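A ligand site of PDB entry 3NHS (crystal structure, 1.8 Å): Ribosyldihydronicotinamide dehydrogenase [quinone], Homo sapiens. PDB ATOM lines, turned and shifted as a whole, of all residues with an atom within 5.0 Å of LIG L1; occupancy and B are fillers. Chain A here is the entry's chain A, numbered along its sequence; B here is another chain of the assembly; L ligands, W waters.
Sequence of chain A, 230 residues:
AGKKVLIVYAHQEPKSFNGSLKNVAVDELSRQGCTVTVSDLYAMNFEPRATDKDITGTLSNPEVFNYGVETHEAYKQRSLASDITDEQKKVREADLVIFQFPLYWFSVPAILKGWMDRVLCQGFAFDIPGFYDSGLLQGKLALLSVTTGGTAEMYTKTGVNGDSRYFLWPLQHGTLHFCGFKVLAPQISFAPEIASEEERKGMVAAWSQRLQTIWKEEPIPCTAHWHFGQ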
ATOM      1  N   HIS A  11     -26.843 -28.653 -18.766  1.00  0.00           N
ATOM      2  CA  HIS A  11     -26.212 -27.401 -19.173  1.00  0.00           C
ATOM      3  C   HIS A  11     -25.988 -27.403 -20.662  1.00  0.00           C
ATOM      4  O   HIS A  11     -25.785 -28.468 -21.268  1.00  0.00           O
ATOM      5  CB  HIS A  11     -24.861 -27.197 -18.392  1.00  0.00           C
ATOM      6  CG  HIS A  11     -24.417 -25.788 -18.371  1.00  0.00           C
ATOM      7  ND1 HIS A  11     -23.907 -25.153 -19.487  1.00  0.00           N
ATOM      8  CD2 HIS A  11     -24.374 -24.870 -17.365  1.00  0.00           C
ATOM      9  CE1 HIS A  11     -23.596 -23.894 -19.157  1.00  0.00           C
ATOM     10  NE2 HIS A  11     -23.884 -23.708 -17.888  1.00  0.00           N
ATOM     11  N   LYS A  15     -18.125 -26.852 -22.466  1.00  0.00           N
ATOM     12  CA  LYS A  15     -16.957 -26.189 -21.854  1.00  0.00           C
ATOM     13  C   LYS A  15     -17.305 -25.408 -20.595  1.00  0.00           C
ATOM     14  O   LYS A  15     -16.413 -24.898 -19.905  1.00  0.00           O
ATOM     15  CB  LYS A  15     -16.221 -25.270 -22.842  1.00  0.00           C
ATOM     16  CG  LYS A  15     -15.647 -25.966 -24.060  1.00  0.00           C
ATOM     17  CD  LYS A  15     -15.065 -24.980 -25.082  1.00  0.00           C
ATOM     18  CE  LYS A  15     -14.593 -25.704 -26.363  1.00  0.00           C
ATOM     19  NZ  LYS A  15     -14.371 -24.700 -27.460  1.00  0.00           N
ATOM     20  N   SER A  16     -18.578 -25.401 -20.220  1.00  0.00           N
ATOM     21  CA  SER A  16     -18.990 -24.764 -18.975  1.00  0.00           C
ATOM     22  C   SER A  16     -18.391 -25.366 -17.752  1.00  0.00           C
ATOM     23  O   SER A  16     -17.891 -26.520 -17.779  1.00  0.00           O
ATOM     24  CB  SER A  16     -20.550 -24.808 -18.831  1.00  0.00           C
ATOM     25  OG  SER A  16     -20.969 -26.160 -18.577  1.00  0.00           O
ATOM     26  N   PHE A  17     -18.448 -24.631 -16.647  1.00  0.00           N
ATOM     27  CA  PHE A  17     -18.144 -25.155 -15.319  1.00  0.00           C
ATOM     28  C   PHE A  17     -19.028 -26.354 -14.914  1.00  0.00           C
ATOM     29  O   PHE A  17     -18.537 -27.298 -14.281  1.00  0.00           O
ATOM     30  CB  PHE A  17     -18.244 -24.091 -14.266  1.00  0.00           C
ATOM     31  CG  PHE A  17     -17.666 -24.469 -12.925  1.00  0.00           C
ATOM     32  CD1 PHE A  17     -16.304 -24.390 -12.715  1.00  0.00           C
ATOM     33  CD2 PHE A  17     -18.474 -24.904 -11.898  1.00  0.00           C
ATOM     34  CE1 PHE A  17     -15.784 -24.740 -11.494  1.00  0.00           C
ATOM     35  CE2 PHE A  17     -17.979 -25.254 -10.692  1.00  0.00           C
ATOM     36  CZ  PHE A  17     -16.613 -25.169 -10.471  1.00  0.00           C
ATOM     37  N   ASN A  18     -20.323 -26.320 -15.265  1.00  0.00           N
ATOM     38  CA  ASN A  18     -21.137 -27.566 -15.034  1.00  0.00           C
ATOM     39  C   ASN A  18     -20.584 -28.746 -15.799  1.00  0.00           C
ATOM     40  O   ASN A  18     -20.602 -29.860 -15.265  1.00  0.00           O
ATOM     41  CB  ASN A  18     -22.608 -27.411 -15.387  1.00  0.00           C
ATOM     42  CG  ASN A  18     -23.408 -26.846 -14.252  1.00  0.00           C
ATOM     43  OD1 ASN A  18     -24.078 -27.607 -13.524  1.00  0.00           O
ATOM     44  ND2 ASN A  18     -23.308 -25.503 -14.036  1.00  0.00           N
ATOM     45  N   SER A  20     -17.457 -29.174 -16.733  1.00  0.00           N
ATOM     46  CA  SER A  20     -16.302 -29.730 -16.055  1.00  0.00           C
ATOM     47  C   SER A  20     -16.681 -30.585 -14.872  1.00  0.00           C
ATOM     48  O   SER A  20     -16.026 -31.641 -14.708  1.00  0.00           O
ATOM     49  CB  SER A  20     -15.317 -28.644 -15.685  1.00  0.00           C
ATOM     50  OG  SER A  20     -14.886 -28.014 -16.878  1.00  0.00           O
ATOM     51  N   PRO A 102     -26.989 -25.807 -13.218  1.00  0.00           N
ATOM     52  CA  PRO A 102     -26.937 -24.426 -12.599  1.00  0.00           C
ATOM     53  C   PRO A 102     -28.287 -24.136 -11.978  1.00  0.00           C
ATOM     54  O   PRO A 102     -29.331 -24.544 -12.524  1.00  0.00           O
ATOM     55  CB  PRO A 102     -26.739 -23.501 -13.788  1.00  0.00           C
ATOM     56  CG  PRO A 102     -27.243 -24.287 -15.002  1.00  0.00           C
ATOM     57  CD  PRO A 102     -27.151 -25.777 -14.685  1.00  0.00           C
ATOM     58  N   LEU A 103     -28.292 -23.445 -10.837  1.00  0.00           N
ATOM     59  CA  LEU A 103     -29.538 -22.983 -10.182  1.00  0.00           C
ATOM     60  C   LEU A 103     -30.219 -21.977 -11.080  1.00  0.00           C
ATOM     61  O   LEU A 103     -29.543 -20.999 -11.492  1.00  0.00           O
ATOM     62  CB  LEU A 103     -29.156 -22.286  -8.887  1.00  0.00           C
ATOM     63  CG  LEU A 103     -30.338 -22.231  -7.898  1.00  0.00           C
ATOM     64  CD1 LEU A 103     -30.891 -23.526  -7.439  1.00  0.00           C
ATOM     65  CD2 LEU A 103     -29.885 -21.470  -6.563  1.00  0.00           C
ATOM     66  N   TYR A 104     -31.482 -22.221 -11.480  1.00  0.00           N
ATOM     67  CA  TYR A 104     -32.264 -21.217 -12.223  1.00  0.00           C
ATOM     68  C   TYR A 104     -33.465 -20.919 -11.359  1.00  0.00           C
ATOM     69  O   TYR A 104     -34.341 -21.817 -11.080  1.00  0.00           O
ATOM     70  CB  TYR A 104     -32.758 -21.817 -13.551  1.00  0.00           C
ATOM     71  CG  TYR A 104     -31.801 -21.810 -14.730  1.00  0.00           C
ATOM     72  CD1 TYR A 104     -30.435 -21.551 -14.646  1.00  0.00           C
ATOM     73  CD2 TYR A 104     -32.312 -22.130 -16.016  1.00  0.00           C
ATOM     74  CE1 TYR A 104     -29.626 -21.615 -15.828  1.00  0.00           C
ATOM     75  CE2 TYR A 104     -31.504 -22.157 -17.124  1.00  0.00           C
ATOM     76  CZ  TYR A 104     -30.183 -21.943 -17.022  1.00  0.00           C
ATOM     77  OH  TYR A 104     -29.431 -21.962 -18.180  1.00  0.00           O
ATOM     78  N   TRP A 105     -33.548 -19.653 -10.888  1.00  0.00           N
ATOM     79  CA  TRP A 105     -34.702 -19.235 -10.066  1.00  0.00           C
ATOM     80  C   TRP A 105     -34.973 -20.132  -8.836  1.00  0.00           C
ATOM     81  O   TRP A 105     -36.115 -20.588  -8.630  1.00  0.00           O
ATOM     82  CB  TRP A 105     -35.957 -19.115 -10.944  1.00  0.00           C
ATOM     83  CG  TRP A 105     -35.848 -18.045 -11.954  1.00  0.00           C
ATOM     84  CD1 TRP A 105     -36.008 -18.159 -13.300  1.00  0.00           C
ATOM     85  CD2 TRP A 105     -35.624 -16.608 -11.686  1.00  0.00           C
ATOM     86  NE1 TRP A 105     -35.807 -16.889 -13.908  1.00  0.00           N
ATOM     87  CE2 TRP A 105     -35.662 -15.938 -12.921  1.00  0.00           C
ATOM     88  CE3 TRP A 105     -35.444 -15.861 -10.505  1.00  0.00           C
ATOM     89  CZ2 TRP A 105     -35.445 -14.536 -13.025  1.00  0.00           C
ATOM     90  CZ3 TRP A 105     -35.242 -14.489 -10.604  1.00  0.00           C
ATOM     91  CH2 TRP A 105     -35.268 -13.838 -11.860  1.00  0.00           C
ATOM     92  N   PHE A 106     -33.867 -20.411  -8.093  1.00  0.00           N
ATOM     93  CA  PHE A 106     -33.858 -21.150  -6.807  1.00  0.00           C
ATOM     94  C   PHE A 106     -34.384 -22.543  -7.087  1.00  0.00           C
ATOM     95  O   PHE A 106     -35.061 -23.175  -6.186  1.00  0.00           O
ATOM     96  CB  PHE A 106     -34.829 -20.461  -5.816  1.00  0.00           C
ATOM     97  CG  PHE A 106     -34.206 -19.328  -4.979  1.00  0.00           C
ATOM     98  CD1 PHE A 106     -33.292 -18.463  -5.530  1.00  0.00           C
ATOM     99  CD2 PHE A 106     -34.637 -19.153  -3.646  1.00  0.00           C
ATOM    100  CE1 PHE A 106     -32.731 -17.429  -4.734  1.00  0.00           C
ATOM    101  CE2 PHE A 106     -34.117 -18.144  -2.818  1.00  0.00           C
ATOM    102  CZ  PHE A 106     -33.182 -17.272  -3.365  1.00  0.00           C
ATOM    103  N   THR A 147     -24.542 -25.511  -9.183  1.00  0.00           N
ATOM    104  CA  THR A 147     -23.726 -24.300  -9.232  1.00  0.00           C
ATOM    105  C   THR A 147     -24.663 -23.054  -9.075  1.00  0.00           C
ATOM    106  O   THR A 147     -25.838 -23.141  -9.434  1.00  0.00           O
ATOM    107  CB  THR A 147     -22.922 -24.187 -10.491  1.00  0.00           C
ATOM    108  OG1 THR A 147     -23.781 -23.971 -11.654  1.00  0.00           O
ATOM    109  CG2 THR A 147     -22.110 -25.480 -10.666  1.00  0.00           C
ATOM    110  N   THR A 148     -24.128 -21.958  -8.533  1.00  0.00           N
ATOM    111  CA  THR A 148     -24.957 -20.754  -8.328  1.00  0.00           C
ATOM    112  C   THR A 148     -24.313 -19.533  -8.879  1.00  0.00           C
ATOM    113  O   THR A 148     -23.090 -19.481  -9.034  1.00  0.00           O
ATOM    114  CB  THR A 148     -25.164 -20.430  -6.869  1.00  0.00           C
ATOM    115  OG1 THR A 148     -23.880 -20.033  -6.330  1.00  0.00           O
ATOM    116  CG2 THR A 148     -25.699 -21.571  -6.108  1.00  0.00           C
ATOM    117  N   GLY A 149     -25.075 -18.472  -9.164  1.00  0.00           N
ATOM    118  CA  GLY A 149     -24.430 -17.229  -9.528  1.00  0.00           C
ATOM    119  C   GLY A 149     -24.034 -16.422  -8.282  1.00  0.00           C
ATOM    120  O   GLY A 149     -23.135 -15.591  -8.328  1.00  0.00           O
ATOM    121  N   GLY A 150     -24.756 -16.587  -7.216  1.00  0.00           N
ATOM    122  CA  GLY A 150     -24.571 -15.719  -6.045  1.00  0.00           C
ATOM    123  C   GLY A 150     -23.676 -16.397  -5.038  1.00  0.00           C
ATOM    124  O   GLY A 150     -23.815 -17.615  -4.802  1.00  0.00           O
ATOM    125  N   TYR A 155     -26.148 -16.613   0.414  1.00  0.00           N
ATOM    126  CA  TYR A 155     -26.948 -17.781   0.827  1.00  0.00           C
ATOM    127  C   TYR A 155     -26.852 -18.170   2.322  1.00  0.00           C
ATOM    128  O   TYR A 155     -27.006 -19.329   2.704  1.00  0.00           O
ATOM    129  CB  TYR A 155     -26.703 -18.997  -0.090  1.00  0.00           C
ATOM    130  CG  TYR A 155     -27.317 -18.838  -1.477  1.00  0.00           C
ATOM    131  CD1 TYR A 155     -28.676 -19.102  -1.672  1.00  0.00           C
ATOM    132  CD2 TYR A 155     -26.545 -18.401  -2.541  1.00  0.00           C
ATOM    133  CE1 TYR A 155     -29.261 -18.943  -2.941  1.00  0.00           C
ATOM    134  CE2 TYR A 155     -27.125 -18.240  -3.840  1.00  0.00           C
ATOM    135  CZ  TYR A 155     -28.467 -18.541  -4.004  1.00  0.00           C
ATOM    136  OH  TYR A 155     -29.062 -18.373  -5.223  1.00  0.00           O
ATOM    137  N   ASN A 161     -30.764 -13.947   0.048  1.00  0.00           N
ATOM    138  CA  ASN A 161     -31.339 -15.138  -0.570  1.00  0.00           C
ATOM    139  C   ASN A 161     -31.878 -16.107   0.450  1.00  0.00           C
ATOM    140  O   ASN A 161     -32.625 -17.042   0.087  1.00  0.00           O
ATOM    141  CB  ASN A 161     -30.288 -15.861  -1.448  1.00  0.00           C
ATOM    142  CG  ASN A 161     -29.873 -15.063  -2.700  1.00  0.00           C
ATOM    143  OD1 ASN A 161     -30.607 -14.218  -3.213  1.00  0.00           O
ATOM    144  ND2 ASN A 161     -28.709 -15.344  -3.181  1.00  0.00           N
ATOM    145  N   PRO A 192     -19.072 -19.619  -9.552  1.00  0.00           N
ATOM    146  CA  PRO A 192     -17.893 -19.793 -10.388  1.00  0.00           C
ATOM    147  C   PRO A 192     -17.639 -18.706 -11.441  1.00  0.00           C
ATOM    148  O   PRO A 192     -16.538 -18.636 -11.985  1.00  0.00           O
ATOM    149  CB  PRO A 192     -18.211 -21.105 -11.133  1.00  0.00           C
ATOM    150  CG  PRO A 192     -19.712 -21.124 -11.190  1.00  0.00           C
ATOM    151  CD  PRO A 192     -20.017 -20.736  -9.784  1.00  0.00           C
ATOM    152  N   GLU A 193     -18.633 -17.898 -11.792  1.00  0.00           N
ATOM    153  CA  GLU A 193     -18.370 -16.979 -12.868  1.00  0.00           C
ATOM    154  C   GLU A 193     -17.368 -15.907 -12.394  1.00  0.00           C
ATOM    155  O   GLU A 193     -16.584 -15.384 -13.193  1.00  0.00           O
ATOM    156  CB  GLU A 193     -19.649 -16.348 -13.399  1.00  0.00           C
ATOM    157  CG  GLU A 193     -20.300 -17.133 -14.518  1.00  0.00           C
ATOM    158  CD  GLU A 193     -21.809 -16.859 -14.612  1.00  0.00           C
ATOM    159  OE1 GLU A 193     -22.582 -17.236 -13.666  1.00  0.00           O
ATOM    160  OE2 GLU A 193     -22.200 -16.263 -15.644  1.00  0.00           O
ATOM    161  N   GLU A 197      -9.617 -18.396 -12.072  1.00  0.00           N
ATOM    162  CA  GLU A 197      -9.232 -19.582 -12.858  1.00  0.00           C
ATOM    163  C   GLU A 197      -8.635 -20.658 -11.931  1.00  0.00           C
ATOM    164  O   GLU A 197      -8.833 -21.857 -12.143  1.00  0.00           O
ATOM    165  CB  GLU A 197      -8.281 -19.167 -13.993  1.00  0.00           C
ATOM    166  CG  GLU A 197      -8.684 -19.703 -15.359  1.00  0.00           C
ATOM    167  CD  GLU A 197      -8.019 -21.039 -15.698  1.00  0.00           C
ATOM    168  OE1 GLU A 197      -8.724 -22.066 -15.847  1.00  0.00           O
ATOM    169  OE2 GLU A 197      -6.778 -21.052 -15.825  1.00  0.00           O
ATOM    170  N   ARG A 200     -11.559 -21.896  -8.990  1.00  0.00           N
ATOM    171  CA  ARG A 200     -12.421 -22.742  -9.826  1.00  0.00           C
ATOM    172  C   ARG A 200     -11.901 -24.199  -9.876  1.00  0.00           C
ATOM    173  O   ARG A 200     -12.651 -25.127 -10.147  1.00  0.00           O
ATOM    174  CB  ARG A 200     -12.569 -22.134 -11.231  1.00  0.00           C
ATOM    175  CG  ARG A 200     -13.568 -20.966 -11.306  1.00  0.00           C
ATOM    176  CD  ARG A 200     -13.954 -20.686 -12.732  1.00  0.00           C
ATOM    177  NE  ARG A 200     -13.388 -19.442 -13.254  1.00  0.00           N
ATOM    178  CZ  ARG A 200     -12.461 -19.355 -14.207  1.00  0.00           C
ATOM    179  NH1 ARG A 200     -11.930 -20.446 -14.753  1.00  0.00           N
ATOM    180  NH2 ARG A 200     -12.031 -18.169 -14.606  1.00  0.00           N
ATOM    181  N   LYS A 201     -10.624 -24.373  -9.560  1.00  0.00           N
ATOM    182  CA  LYS A 201      -9.999 -25.698  -9.426  1.00  0.00           C
ATOM    183  C   LYS A 201     -10.209 -26.340  -8.060  1.00  0.00           C
ATOM    184  O   LYS A 201     -10.411 -27.550  -7.948  1.00  0.00           O
ATOM    185  CB  LYS A 201      -8.500 -25.607  -9.751  1.00  0.00           C
ATOM    186  CG  LYS A 201      -8.161 -24.960 -11.112  1.00  0.00           C
ATOM    187  CD  LYS A 201      -8.897 -25.620 -12.256  1.00  0.00           C
ATOM    188  CE  LYS A 201      -8.028 -25.775 -13.516  1.00  0.00           C
ATOM    189  NZ  LYS A 201      -7.279 -24.545 -13.933  1.00  0.00           N
ATOM    190  N   VAL A 204     -13.710 -27.954  -8.261  1.00  0.00           N
ATOM    191  CA  VAL A 204     -13.664 -29.171  -9.113  1.00  0.00           C
ATOM    192  C   VAL A 204     -12.952 -30.320  -8.365  1.00  0.00           C
ATOM    193  O   VAL A 204     -13.435 -31.433  -8.378  1.00  0.00           O
ATOM    194  CB  VAL A 204     -13.064 -28.879 -10.507  1.00  0.00           C
ATOM    195  CG1 VAL A 204     -13.016 -30.099 -11.410  1.00  0.00           C
ATOM    196  CG2 VAL A 204     -13.876 -27.859 -11.204  1.00  0.00           C
ATOM    197  N   VAL B  64     -17.831 -20.193 -26.113  1.00  0.00           N
ATOM    198  CA  VAL B  64     -18.343 -20.727 -24.846  1.00  0.00           C
ATOM    199  C   VAL B  64     -19.689 -20.029 -24.536  1.00  0.00           C
ATOM    200  O   VAL B  64     -19.725 -18.868 -24.147  1.00  0.00           O
ATOM    201  CB  VAL B  64     -17.314 -20.516 -23.696  1.00  0.00           C
ATOM    202  CG1 VAL B  64     -17.841 -21.042 -22.350  1.00  0.00           C
ATOM    203  CG2 VAL B  64     -15.942 -21.174 -24.038  1.00  0.00           C
ATOM    204  N   ASN B  66     -22.980 -18.935 -22.759  1.00  0.00           N
ATOM    205  CA  ASN B  66     -23.446 -18.664 -21.403  1.00  0.00           C
ATOM    206  C   ASN B  66     -24.822 -18.022 -21.574  1.00  0.00           C
ATOM    207  O   ASN B  66     -24.915 -16.911 -22.128  1.00  0.00           O
ATOM    208  CB  ASN B  66     -22.466 -17.695 -20.718  1.00  0.00           C
ATOM    209  CG  ASN B  66     -22.848 -17.392 -19.354  1.00  0.00           C
ATOM    210  OD1 ASN B  66     -24.028 -17.105 -19.060  1.00  0.00           O
ATOM    211  ND2 ASN B  66     -21.840 -17.420 -18.434  1.00  0.00           N
ATOM    212  N   TYR B  67     -25.871 -18.739 -21.168  1.00  0.00           N
ATOM    213  CA  TYR B  67     -27.232 -18.381 -21.524  1.00  0.00           C
ATOM    214  C   TYR B  67     -27.526 -17.011 -20.868  1.00  0.00           C
ATOM    215  O   TYR B  67     -28.154 -16.156 -21.524  1.00  0.00           O
ATOM    216  CB  TYR B  67     -28.238 -19.385 -20.961  1.00  0.00           C
ATOM    217  CG  TYR B  67     -29.668 -19.046 -21.372  1.00  0.00           C
ATOM    218  CD1 TYR B  67     -30.116 -19.303 -22.693  1.00  0.00           C
ATOM    219  CD2 TYR B  67     -30.574 -18.460 -20.480  1.00  0.00           C
ATOM    220  CE1 TYR B  67     -31.416 -19.030 -23.095  1.00  0.00           C
ATOM    221  CE2 TYR B  67     -31.864 -18.140 -20.938  1.00  0.00           C
ATOM    222  CZ  TYR B  67     -32.260 -18.454 -22.223  1.00  0.00           C
ATOM    223  OH  TYR B  67     -33.519 -18.142 -22.656  1.00  0.00           O
ATOM    224  N   GLY B  68     -27.137 -16.808 -19.604  1.00  0.00           N
ATOM    225  CA  GLY B  68     -27.435 -15.512 -18.914  1.00  0.00           C
ATOM    226  C   GLY B  68     -26.735 -14.302 -19.567  1.00  0.00           C
ATOM    227  O   GLY B  68     -27.357 -13.237 -19.826  1.00  0.00           O
ATOM    228  N   ASP B 117     -37.814 -18.955 -16.759  1.00  0.00           N
ATOM    229  CA  ASP B 117     -36.393 -18.960 -17.076  1.00  0.00           C
ATOM    230  C   ASP B 117     -36.111 -18.046 -18.251  1.00  0.00           C
ATOM    231  O   ASP B 117     -35.052 -17.384 -18.323  1.00  0.00           O
ATOM    232  CB  ASP B 117     -36.016 -20.417 -17.478  1.00  0.00           C
ATOM    233  CG  ASP B 117     -35.992 -21.398 -16.272  1.00  0.00           C
ATOM    234  OD1 ASP B 117     -36.078 -21.015 -15.040  1.00  0.00           O
ATOM    235  OD2 ASP B 117     -35.836 -22.572 -16.610  1.00  0.00           O
HETATM  236  P1  LIG L   1     -19.756 -20.958 -16.503  1.00  0.00           P
HETATM  237  O1  LIG L   1     -19.945 -19.512 -16.944  1.00  0.00           O
HETATM  238  O2  LIG L   1     -19.882 -21.895 -17.669  1.00  0.00           O
HETATM  239  O3  LIG L   1     -18.309 -21.175 -15.823  1.00  0.00           O
HETATM  240  C1  LIG L   1     -17.570 -20.314 -14.988  1.00  0.00           C
HETATM  241  C2  LIG L   1     -16.156 -20.316 -15.612  1.00  0.00           C
HETATM  242  O4  LIG L   1     -15.477 -21.546 -15.398  1.00  0.00           O
HETATM  243  C3  LIG L   1     -16.160 -20.140 -17.139  1.00  0.00           C
HETATM  244  O5  LIG L   1     -15.346 -19.035 -17.464  1.00  0.00           O
HETATM  245  C4  LIG L   1     -15.608 -21.433 -17.730  1.00  0.00           C
HETATM  246  O6  LIG L   1     -14.815 -21.336 -18.891  1.00  0.00           O
HETATM  247  C5  LIG L   1     -14.755 -21.862 -16.577  1.00  0.00           C
HETATM  248  N1  LIG L   1     -14.438 -23.281 -16.589  1.00  0.00           N
HETATM  249  C6  LIG L   1     -14.923 -24.306 -17.370  1.00  0.00           C
HETATM  250  N2  LIG L   1     -14.297 -25.439 -16.964  1.00  0.00           N
HETATM  251  C7  LIG L   1     -13.439 -25.133 -15.950  1.00  0.00           C
HETATM  252  C8  LIG L   1     -12.549 -25.886 -15.175  1.00  0.00           C
HETATM  253  N3  LIG L   1     -12.223 -27.129 -15.528  1.00  0.00           N
HETATM  254  N4  LIG L   1     -11.804 -25.249 -14.185  1.00  0.00           N
HETATM  255  C9  LIG L   1     -11.912 -23.893 -13.976  1.00  0.00           C
HETATM  256  N5  LIG L   1     -12.778 -23.174 -14.759  1.00  0.00           N
HETATM  257  C10 LIG L   1     -13.525 -23.779 -15.706  1.00  0.00           C
HETATM  258  N6  LIG L   1     -27.986 -17.888  -9.544  1.00  0.00           N
HETATM  259  C11 LIG L   1     -28.399 -17.935  -8.267  1.00  0.00           C
HETATM  260  O7  LIG L   1     -27.595 -17.897  -7.308  1.00  0.00           O
HETATM  261  N7  LIG L   1     -29.744 -18.045  -7.987  1.00  0.00           N
HETATM  262  C12 LIG L   1     -30.690 -18.168  -9.021  1.00  0.00           C
HETATM  263  O8  LIG L   1     -31.896 -18.298  -8.676  1.00  0.00           O
HETATM  264  C13 LIG L   1     -30.257 -18.046 -10.339  1.00  0.00           C
HETATM  265  N8  LIG L   1     -31.193 -18.090 -11.395  1.00  0.00           N
HETATM  266  C14 LIG L   1     -30.769 -18.033 -12.700  1.00  0.00           C
HETATM  267  C15 LIG L   1     -31.769 -18.130 -13.752  1.00  0.00           C
HETATM  268  C16 LIG L   1     -31.312 -18.128 -15.065  1.00  0.00           C
HETATM  269  C17 LIG L   1     -32.387 -18.232 -16.143  1.00  0.00           C
HETATM  270  C18 LIG L   1     -29.960 -17.987 -15.383  1.00  0.00           C
HETATM  271  C19 LIG L   1     -29.491 -17.944 -16.844  1.00  0.00           C
HETATM  272  C20 LIG L   1     -29.014 -17.963 -14.337  1.00  0.00           C
HETATM  273  C21 LIG L   1     -29.431 -17.936 -13.013  1.00  0.00           C
HETATM  274  N9  LIG L   1     -28.475 -17.899 -11.944  1.00  0.00           N
HETATM  275  C22 LIG L   1     -28.909 -17.979 -10.623  1.00  0.00           C
HETATM  276  C23 LIG L   1     -27.023 -17.835 -12.321  1.00  0.00           C
HETATM  277  C24 LIG L   1     -26.500 -19.311 -12.575  1.00  0.00           C
HETATM  278  O9  LIG L   1     -26.898 -20.233 -11.545  1.00  0.00           O
HETATM  279  C25 LIG L   1     -25.005 -19.265 -12.874  1.00  0.00           C
HETATM  280  O10 LIG L   1     -24.791 -18.478 -14.012  1.00  0.00           O
HETATM  281  C26 LIG L   1     -24.381 -20.640 -13.183  1.00  0.00           C
HETATM  282  O11 LIG L   1     -24.551 -21.425 -12.047  1.00  0.00           O
HETATM  283  C27 LIG L   1     -22.853 -20.630 -13.459  1.00  0.00           C
HETATM  284  O12 LIG L   1     -22.389 -22.027 -13.758  1.00  0.00           O
HETATM  285  P2  LIG L   1     -21.963 -22.254 -15.250  1.00  0.00           P
HETATM  286  O13 LIG L   1     -23.011 -21.904 -16.314  1.00  0.00           O
HETATM  287  O14 LIG L   1     -21.564 -23.696 -15.464  1.00  0.00           O
HETATM  288  O15 LIG L   1     -20.624 -21.268 -15.211  1.00  0.00           O
HETATM  289  C1  LG2 L   2     -28.273 -14.486  -8.548  1.00  0.00           C
HETATM  290  C2  LG2 L   2     -29.272 -14.588  -9.530  1.00  0.00           C
HETATM  291  C3  LG2 L   2     -28.898 -14.473 -10.879  1.00  0.00           C
HETATM  292  C4  LG2 L   2     -27.580 -14.301 -11.251  1.00  0.00           C
HETATM  293  C5  LG2 L   2     -26.580 -14.213 -10.271  1.00  0.00           C
HETATM  294  C6  LG2 L   2     -26.940 -14.298  -8.927  1.00  0.00           C
HETATM  295  C7  LG2 L   2     -30.726 -14.785  -9.277  1.00  0.00           C
HETATM  296  C8  LG2 L   2     -31.580 -14.831 -10.349  1.00  0.00           C
HETATM  297  C9  LG2 L   2     -31.105 -14.718 -11.618  1.00  0.00           C
HETATM  298  N1  LG2 L   2     -29.798 -14.542 -11.860  1.00  0.00           N
HETATM  299  O1  LG2 L   2     -28.659 -14.614  -7.212  1.00  0.00           O
HETATM  300  O2  LG2 L   2     -27.411 -14.186 -12.619  1.00  0.00           O
HETATM  301  C10 LG2 L   2     -26.210 -14.429 -13.375  1.00  0.00           C
HETATM  302  C11 LG2 L   2     -27.820 -14.432  -6.080  1.00  0.00           C
HETATM  303  C12 LG2 L   2     -31.431 -14.933  -7.961  1.00  0.00           C
HETATM  304  O3  LG2 L   2     -31.941 -14.788 -12.556  1.00  0.00           O
HETATM  305  O   HOH W   1     -34.012 -15.547 -16.449  1.00  0.00           O
HETATM  306  O   HOH W   2     -26.099 -18.489 -17.146  1.00  0.00           O
HETATM  307  O   HOH W   3     -12.121 -23.640 -18.505  1.00  0.00           O
HETATM  308  O   HOH W   4     -21.156 -21.686 -20.063  1.00  0.00           O
HETATM  309  O   HOH W   5     -19.128 -18.534 -19.739  1.00  0.00           O
HETATM  310  O   HOH W   6     -25.666 -21.163 -16.663  1.00  0.00           O
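ND1 of His 11 sits at hydrogen-bond distance from OG of Ser 16 (3.2 Å).
ND2 of Asn 66 of chain B lies within hydrogen-bond range of OE2 of Glu 193 (3.0 Å).
The backbone carbonyl oxygen (O) of Ser 16 sits at hydrogen-bond distance from the side-chain hydroxyl (OG) of Ser 20, at 3.5 Å.
The backbone NH of Leu 103 lies within hydrogen-bond range of the backbone carbonyl oxygen of Thr 147 (2.8 Å).
The side-chain amide nitrogen (ND2) of Asn 18 is in hydrogen-bond range of the side-chain hydroxyl (OG1) of Thr 147.
NE of Arg 200 sits close to O of Pro 192 (3.5 Å).
The side-chain amide oxygen (OD1) of Asn 66 of chain B lies within hydrogen-bond range of the backbone NH (N) of Gly 68 of chain B, at 3.2 Å.
OE1 of Glu 197 is in salt-bridge range of NZ of Lys 201 (3.4 Å).
Residues that only touch LIG L1: Lys 15, Ser 16, Tyr 104, Pro 102, Lys 201, Thr 148, Asp 117 of chain B, Pro 192, Gly 68 of chain B and Tyr 67 of chain B.
Within 4 Å of LIG L1: His 11, Lys 15, Ser 16, Phe 17, Asn 18, Ser 20, Pro 102, Leu 103, Tyr 104, Trp 105, Phe 106, Thr 147, Thr 148, Gly 149, Gly 150, Tyr 155, Pro 192, Glu 193, Arg 200, Lys 201, Asn 66 of chain B, Tyr 67 of chain B, Gly 68 of chain B and Asp 117 of chain B.
The nearest printed residue that does not touch LIG L1 is Glu 197 (4.1 Å).
Water W6 lies within hydrogen-bond range of an oxygen (O13) of LIG L1 (2.8 Å) and a ring nitrogen (NE2) of His 11 (3.3 Å).
Water W5 lies within hydrogen-bond range of O1 of LIG L1 (3.1 Å) and ND2 of Asn 66 of chain B (3.2 Å).
Water W1 bridges the backbone carbonyl oxygen of Asp 117 of chain B (2.8 Å) and the indole nitrogen of Trp 105 (3.4 Å).
Water W2 lies within hydrogen-bond range of OD1 of Asn 66 of chain B (3.1 Å), N of Gly 68 of chain B (3.2 Å) and O10 of LIG L1 (3.4 Å).
A ring nitrogen (NE2) of His 11 is in hydrogen-bond range of an oxygen (O13) of LIG L1, at 2.5 Å.
An oxygen (O10) of LIG L1 lies within hydrogen-bond range of the side-chain carboxylate (OE1) of Glu 193 (2.6 Å).
The side-chain hydroxyl of Tyr 155 sits at hydrogen-bond distance from an oxygen (O7) of LIG L1, 2.6 Å away.
A nitrogen (N2) of LIG L1 lies within hydrogen-bond range of the side-chain hydroxyl of Ser 20 (2.6 Å).
The backbone carbonyl oxygen of Thr 147 sits at hydrogen-bond distance from an oxygen (O11) of LIG L1 (3.4 Å).
O11 of LIG L1 sits at hydrogen-bond distance from OG1 of Thr 147 (2.7 Å).
The backbone carbonyl oxygen (O) of Leu 103 lies within hydrogen-bond range of an oxygen (O9) of LIG L1, at 2.8 Å.
NH1 of Arg 200 is in hydrogen-bond range of N5 of LIG L1, 2.9 Å away.
N of Trp 105 lies within hydrogen-bond range of N8 of LIG L1.
The backbone NH (N) of Asn 18 lies within hydrogen-bond range of an oxygen (O14) of LIG L1.
O14 of LIG L1 is in hydrogen-bond range of ND2 of Asn 18 (2.9 Å).
O8 of LIG L1 lies within hydrogen-bond range of N of Phe 106.
The backbone NH of Gly 149 sits at hydrogen-bond distance from a nitrogen (N6) of LIG L1, 3.0 Å away.
N of Gly 150 is in hydrogen-bond range of O7 of LIG L1 (3.1 Å).
ND2 of Asn 66 of chain B sits at hydrogen-bond distance from O1 of LIG L1 (3.2 Å).
The backbone NH of Phe 17 sits at hydrogen-bond distance from an oxygen (O2) of LIG L1, at 3.3 Å.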
